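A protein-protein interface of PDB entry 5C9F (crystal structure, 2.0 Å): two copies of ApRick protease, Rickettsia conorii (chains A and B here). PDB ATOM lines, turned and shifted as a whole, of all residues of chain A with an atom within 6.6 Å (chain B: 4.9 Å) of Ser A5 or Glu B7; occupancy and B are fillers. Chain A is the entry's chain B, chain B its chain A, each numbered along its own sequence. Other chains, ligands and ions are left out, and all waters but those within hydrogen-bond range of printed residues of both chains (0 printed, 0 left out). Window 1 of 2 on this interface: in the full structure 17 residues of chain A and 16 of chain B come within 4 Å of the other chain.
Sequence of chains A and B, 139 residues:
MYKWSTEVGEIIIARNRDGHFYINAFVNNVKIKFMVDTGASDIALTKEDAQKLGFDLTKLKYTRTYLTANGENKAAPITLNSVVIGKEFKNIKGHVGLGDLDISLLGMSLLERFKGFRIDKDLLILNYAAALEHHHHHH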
ATOM      1  N   LYS A   3     -32.668 -11.624 -11.044  1.00  0.00           N
ATOM      2  CA  LYS A   3     -31.548 -10.807 -11.303  1.00  0.00           C
ATOM      3  C   LYS A   3     -30.776 -11.374 -12.487  1.00  0.00           C
ATOM      4  O   LYS A   3     -30.523 -12.560 -12.591  1.00  0.00           O
ATOM      5  CB  LYS A   3     -30.650 -10.756 -10.090  1.00  0.00           C
ATOM      6  CG  LYS A   3     -29.502  -9.787 -10.197  1.00  0.00           C
ATOM      7  CD  LYS A   3     -28.785  -9.703  -8.850  1.00  0.00           C
ATOM      8  CE  LYS A   3     -27.661  -8.679  -8.855  1.00  0.00           C
ATOM      9  NZ  LYS A   3     -26.502  -9.086  -9.695  1.00  0.00           N
ATOM     10  N   TRP A   4     -30.363 -10.483 -13.360  1.00  0.00           N
ATOM     11  CA  TRP A   4     -29.551 -10.851 -14.532  1.00  0.00           C
ATOM     12  C   TRP A   4     -28.572  -9.723 -14.709  1.00  0.00           C
ATOM     13  O   TRP A   4     -28.924  -8.549 -14.534  1.00  0.00           O
ATOM     14  CB  TRP A   4     -30.481 -10.979 -15.784  1.00  0.00           C
ATOM     15  CG  TRP A   4     -29.683 -11.038 -17.081  1.00  0.00           C
ATOM     16  CD1 TRP A   4     -29.274  -9.962 -17.846  1.00  0.00           C
ATOM     17  CD2 TRP A   4     -29.130 -12.206 -17.714  1.00  0.00           C
ATOM     18  NE1 TRP A   4     -28.524 -10.398 -18.911  1.00  0.00           N
ATOM     19  CE2 TRP A   4     -28.418 -11.763 -18.860  1.00  0.00           C
ATOM     20  CE3 TRP A   4     -29.174 -13.575 -17.433  1.00  0.00           C
ATOM     21  CZ2 TRP A   4     -27.755 -12.640 -19.715  1.00  0.00           C
ATOM     22  CZ3 TRP A   4     -28.530 -14.446 -18.301  1.00  0.00           C
ATOM     23  CH2 TRP A   4     -27.816 -13.972 -19.423  1.00  0.00           C
ATOM     24  N   SER A   5     -27.366 -10.028 -15.138  1.00  0.00           N
ATOM     25  CA  SER A   5     -26.471  -8.977 -15.583  1.00  0.00           C
ATOM     26  C   SER A   5     -25.549  -9.383 -16.742  1.00  0.00           C
ATOM     27  O   SER A   5     -25.259 -10.552 -16.921  1.00  0.00           O
ATOM     28  CB  SER A   5     -25.661  -8.431 -14.424  1.00  0.00           C
ATOM     29  OG  SER A   5     -24.742  -9.362 -13.922  1.00  0.00           O
ATOM     30  N   THR A   6     -25.138  -8.375 -17.510  1.00  0.00           N
ATOM     31  CA  THR A   6     -24.226  -8.501 -18.646  1.00  0.00           C
ATOM     32  C   THR A   6     -23.024  -7.589 -18.392  1.00  0.00           C
ATOM     33  O   THR A   6     -23.178  -6.414 -18.073  1.00  0.00           O
ATOM     34  CB  THR A   6     -24.853  -7.972 -19.948  1.00  0.00           C
ATOM     35  OG1 THR A   6     -26.122  -8.549 -20.188  1.00  0.00           O
ATOM     36  CG2 THR A   6     -23.959  -8.231 -21.148  1.00  0.00           C
ATOM     37  N   GLU A   7     -21.827  -8.106 -18.575  1.00  0.00           N
ATOM     38  CA  GLU A   7     -20.619  -7.262 -18.612  1.00  0.00           C
ATOM     39  C   GLU A   7     -20.342  -6.780 -20.058  1.00  0.00           C
ATOM     40  O   GLU A   7     -20.207  -7.589 -20.961  1.00  0.00           O
ATOM     41  CB  GLU A   7     -19.412  -8.023 -18.111  1.00  0.00           C
ATOM     42  CG  GLU A   7     -18.168  -7.150 -18.051  1.00  0.00           C
ATOM     43  CD  GLU A   7     -16.863  -7.911 -17.863  1.00  0.00           C
ATOM     44  OE1 GLU A   7     -16.834  -9.134 -18.065  1.00  0.00           O
ATOM     45  OE2 GLU A   7     -15.846  -7.267 -17.538  1.00  0.00           O
ATOM     46  N   VAL A   8     -20.331  -5.458 -20.274  1.00  0.00           N
ATOM     47  CA  VAL A   8     -20.113  -4.848 -21.575  1.00  0.00           C
ATOM     48  C   VAL A   8     -18.764  -4.194 -21.488  1.00  0.00           C
ATOM     49  O   VAL A   8     -18.535  -3.327 -20.648  1.00  0.00           O
ATOM     50  CB  VAL A   8     -21.185  -3.778 -21.928  1.00  0.00           C
ATOM     51  CG1 VAL A   8     -20.897  -3.216 -23.317  1.00  0.00           C
ATOM     52  CG2 VAL A   8     -22.558  -4.396 -21.938  1.00  0.00           C
ATOM     53  N   ALA A 130     -20.656 -10.115 -22.338  1.00  0.00           N
ATOM     54  CA  ALA A 130     -20.646 -11.447 -21.726  1.00  0.00           C
ATOM     55  C   ALA A 130     -21.791 -11.519 -20.744  1.00  0.00           C
ATOM     56  O   ALA A 130     -21.947 -10.607 -19.932  1.00  0.00           O
ATOM     57  CB  ALA A 130     -19.327 -11.663 -21.011  1.00  0.00           C
ATOM     58  N   ALA A 131     -22.613 -12.579 -20.823  1.00  0.00           N
ATOM     59  CA  ALA A 131     -23.628 -12.850 -19.789  1.00  0.00           C
ATOM     60  C   ALA A 131     -22.938 -13.074 -18.461  1.00  0.00           C
ATOM     61  O   ALA A 131     -21.802 -13.527 -18.434  1.00  0.00           O
ATOM     62  CB  ALA A 131     -24.494 -14.052 -20.122  1.00  0.00           C
ATOM     63  N   LEU A 132     -23.608 -12.733 -17.365  1.00  0.00           N
ATOM     64  CA  LEU A 132     -23.129 -13.123 -16.046  1.00  0.00           C
ATOM     65  C   LEU A 132     -24.227 -13.890 -15.395  1.00  0.00           C
ATOM     66  O   LEU A 132     -24.029 -14.322 -14.276  1.00  0.00           O
ATOM     67  CB  LEU A 132     -22.770 -11.920 -15.173  1.00  0.00           C
ATOM     68  CG  LEU A 132     -21.398 -11.287 -15.413  1.00  0.00           C
ATOM     69  CD1 LEU A 132     -21.374  -9.839 -14.920  1.00  0.00           C
ATOM     70  CD2 LEU A 132     -20.297 -12.087 -14.738  1.00  0.00           C
ATOM     71  N   SER B   5     -14.547  -2.076 -18.541  1.00  0.00           N
ATOM     72  CA  SER B   5     -15.828  -2.790 -18.595  1.00  0.00           C
ATOM     73  C   SER B   5     -16.835  -2.284 -17.580  1.00  0.00           C
ATOM     74  O   SER B   5     -16.468  -1.790 -16.518  1.00  0.00           O
ATOM     75  CB  SER B   5     -15.668  -4.301 -18.469  1.00  0.00           C
ATOM     76  OG  SER B   5     -15.239  -4.702 -17.165  1.00  0.00           O
ATOM     77  N   THR B   6     -18.108  -2.461 -17.934  1.00  0.00           N
ATOM     78  CA  THR B   6     -19.265  -2.077 -17.126  1.00  0.00           C
ATOM     79  C   THR B   6     -20.167  -3.293 -16.929  1.00  0.00           C
ATOM     80  O   THR B   6     -20.487  -3.998 -17.915  1.00  0.00           O
ATOM     81  CB  THR B   6     -20.140  -1.047 -17.914  1.00  0.00           C
ATOM     82  OG1 THR B   6     -19.354   0.055 -18.368  1.00  0.00           O
ATOM     83  CG2 THR B   6     -21.267  -0.516 -17.065  1.00  0.00           C
ATOM     84  N   GLU B   7     -20.633  -3.514 -15.719  1.00  0.00           N
ATOM     85  CA  GLU B   7     -21.724  -4.462 -15.470  1.00  0.00           C
ATOM     86  C   GLU B   7     -23.096  -3.779 -15.631  1.00  0.00           C
ATOM     87  O   GLU B   7     -23.387  -2.809 -14.923  1.00  0.00           O
ATOM     88  CB  GLU B   7     -21.626  -5.035 -14.079  1.00  0.00           C
ATOM     89  CG  GLU B   7     -22.680  -6.112 -13.815  1.00  0.00           C
ATOM     90  CD  GLU B   7     -22.779  -6.562 -12.360  1.00  0.00           C
ATOM     91  OE1 GLU B   7     -22.286  -5.860 -11.466  1.00  0.00           O
ATOM     92  OE2 GLU B   7     -23.405  -7.598 -12.097  1.00  0.00           O
ATOM     93  N   VAL B   8     -23.919  -4.256 -16.573  1.00  0.00           N
ATOM     94  CA  VAL B   8     -25.263  -3.687 -16.847  1.00  0.00           C
ATOM     95  C   VAL B   8     -26.224  -4.741 -16.374  1.00  0.00           C
ATOM     96  O   VAL B   8     -26.169  -5.891 -16.812  1.00  0.00           O
ATOM     97  CB  VAL B   8     -25.531  -3.427 -18.308  1.00  0.00           C
ATOM     98  CG1 VAL B   8     -26.929  -2.872 -18.508  1.00  0.00           C
ATOM     99  CG2 VAL B   8     -24.515  -2.437 -18.861  1.00  0.00           C
ATOM    100  N   GLY B   9     -27.056  -4.380 -15.432  1.00  0.00           N
ATOM    101  CA  GLY B   9     -27.865  -5.395 -14.739  1.00  0.00           C
ATOM    102  C   GLY B   9     -29.298  -4.975 -14.513  1.00  0.00           C
ATOM    103  O   GLY B   9     -29.633  -3.797 -14.687  1.00  0.00           O
ATOM    104  N   GLY B  86     -28.018  -4.968  -6.443  1.00  0.00           N
ATOM    105  CA  GLY B  86     -27.390  -5.073  -7.758  1.00  0.00           C
ATOM    106  C   GLY B  86     -26.056  -4.353  -7.750  1.00  0.00           C
ATOM    107  O   GLY B  86     -24.997  -4.980  -7.714  1.00  0.00           O
ATOM    108  N   TYR B 128     -29.517  -1.021 -13.706  1.00  0.00           N
ATOM    109  CA  TYR B 128     -28.324  -0.326 -13.233  1.00  0.00           C
ATOM    110  C   TYR B 128     -27.138  -0.564 -14.128  1.00  0.00           C
ATOM    111  O   TYR B 128     -27.126  -1.520 -14.932  1.00  0.00           O
ATOM    112  CB  TYR B 128     -27.953  -0.731 -11.784  1.00  0.00           C
ATOM    113  CG  TYR B 128     -27.629  -2.180 -11.638  1.00  0.00           C
ATOM    114  CD1 TYR B 128     -28.642  -3.088 -11.400  1.00  0.00           C
ATOM    115  CD2 TYR B 128     -26.325  -2.653 -11.729  1.00  0.00           C
ATOM    116  CE1 TYR B 128     -28.379  -4.436 -11.313  1.00  0.00           C
ATOM    117  CE2 TYR B 128     -26.036  -4.018 -11.608  1.00  0.00           C
ATOM    118  CZ  TYR B 128     -27.079  -4.888 -11.393  1.00  0.00           C
ATOM    119  OH  TYR B 128     -26.904  -6.270 -11.305  1.00  0.00           O
ATOM    120  N   ALA B 129     -26.147   0.300 -13.984  1.00  0.00           N
ATOM    121  CA  ALA B 129     -24.847   0.101 -14.608  1.00  0.00           C
ATOM    122  C   ALA B 129     -23.751   0.493 -13.624  1.00  0.00           C
ATOM    123  O   ALA B 129     -23.783   1.567 -13.051  1.00  0.00           O
ATOM    124  CB  ALA B 129     -24.763   0.917 -15.871  1.00  0.00           C
ATOM    125  N   ALA B 130     -22.794  -0.392 -13.420  1.00  0.00           N
ATOM    126  CA  ALA B 130     -21.710  -0.193 -12.472  1.00  0.00           C
ATOM    127  C   ALA B 130     -20.386  -0.338 -13.209  1.00  0.00           C
ATOM    128  O   ALA B 130     -20.231  -1.286 -13.964  1.00  0.00           O
ATOM    129  CB  ALA B 130     -21.825  -1.246 -11.384  1.00  0.00           C
ATOM    130  N   LEU B 132     -16.555  -1.468 -13.823  1.00  0.00           N
ATOM    131  CA  LEU B 132     -15.913  -2.783 -13.530  1.00  0.00           C
ATOM    132  C   LEU B 132     -16.969  -3.876 -13.269  1.00  0.00           C
ATOM    133  O   LEU B 132     -17.210  -4.764 -14.105  1.00  0.00           O
ATOM    134  CB  LEU B 132     -14.896  -2.732 -12.369  1.00  0.00           C
ATOM    135  CG  LEU B 132     -13.397  -2.530 -12.649  1.00  0.00           C
ATOM    136  CD1 LEU B 132     -12.648  -2.110 -11.387  1.00  0.00           C
ATOM    137  CD2 LEU B 132     -12.769  -3.789 -13.230  1.00  0.00           C
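OG of Ser B5 sits at hydrogen-bond distance from OE2 of Glu A7 (2.7 Å).
The backbone carbonyl oxygen (O) of Thr B6 sits at hydrogen-bond distance from the backbone NH (N) of Val A8, at 2.8 Å.
The side-chain carboxylate of Glu B7 is in hydrogen-bond range of the side-chain hydroxyl of Ser A5, 2.9 Å away.
The backbone NH (N) of Val B8 sits at hydrogen-bond distance from the backbone carbonyl oxygen (O) of Thr A6.
The side-chain hydroxyl (OH) of Tyr B128 sits at hydrogen-bond distance from the side-chain amino group (NZ) of Lys A3, at 3.3 Å.
Among the printed residues, pairs that only touch across the chains: Trp A4 with Gly B9, Ser A5 with Val B8, Glu A7 with Thr B6, Val A8 with Ser B5, Thr A6 with Glu B7, Thr A6 with Thr B6, Ser A5 with Gly B9, Lys A3 with Gly B86 and Ser A5 with Tyr B128.
N of Leu B132 sits at hydrogen-bond distance from O of Ser B5, 2.7 Å away.
The backbone carbonyl oxygen (O) of Ala B130 is in hydrogen-bond range of the backbone NH (N) of Glu B7 (2.9 Å).
The backbone NH of Gly B9 is in hydrogen-bond range of the backbone carbonyl oxygen of Tyr B128, 2.9 Å away.
NE1 of Trp A4 is in hydrogen-bond range of OG1 of Thr A6, 3.3 Å away.
The backbone NH of Leu A132 lies within hydrogen-bond range of the backbone carbonyl oxygen of Ser A5.
O of Ala A130 sits at hydrogen-bond distance from N of Glu A7 (2.8 Å).
Ser A5 touches Glu B7, and with the chains exchanged Glu A7 touches Ser B5.
Ser A5 touches Val B8, and with the chains exchanged Val A8 touches Ser B5.
Thr A6 touches its own counterpart, Thr B6.
Thr A6 touches Glu B7, and with the chains exchanged Glu A7 touches Thr B6.
Of the printed residues of chain B, Ser A5 touches Glu B7, Val B8, Gly B9 and Tyr B128.
Of the printed residues of chain B, Val A8 touches Ser B5 and Thr B6.
Of the printed residues of chain A, Thr B6 touches Thr A6, Glu A7 and Val A8.
Of the printed residues of chain A, Tyr B128 touches Lys A3 (3.3 Å) and Ser A5 (3.99 Å).
Printed residues of chain B within 4 Å of Thr A6: Thr B6, Glu B7 and Val B8.
Ala A130 touches none of the printed residues of chain B.
Leu B132 touches none of the printed residues of chain A.
The nearest residue of chain A that does not touch Glu B7 is Leu A132 (4.1 Å).
Hydrophobic or aromatic side chains of chain B that line the printed part of chain A: Val B8 and Tyr B128.
Of the 9 printed residues of chain A, 6 touch a printed residue of chain B.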
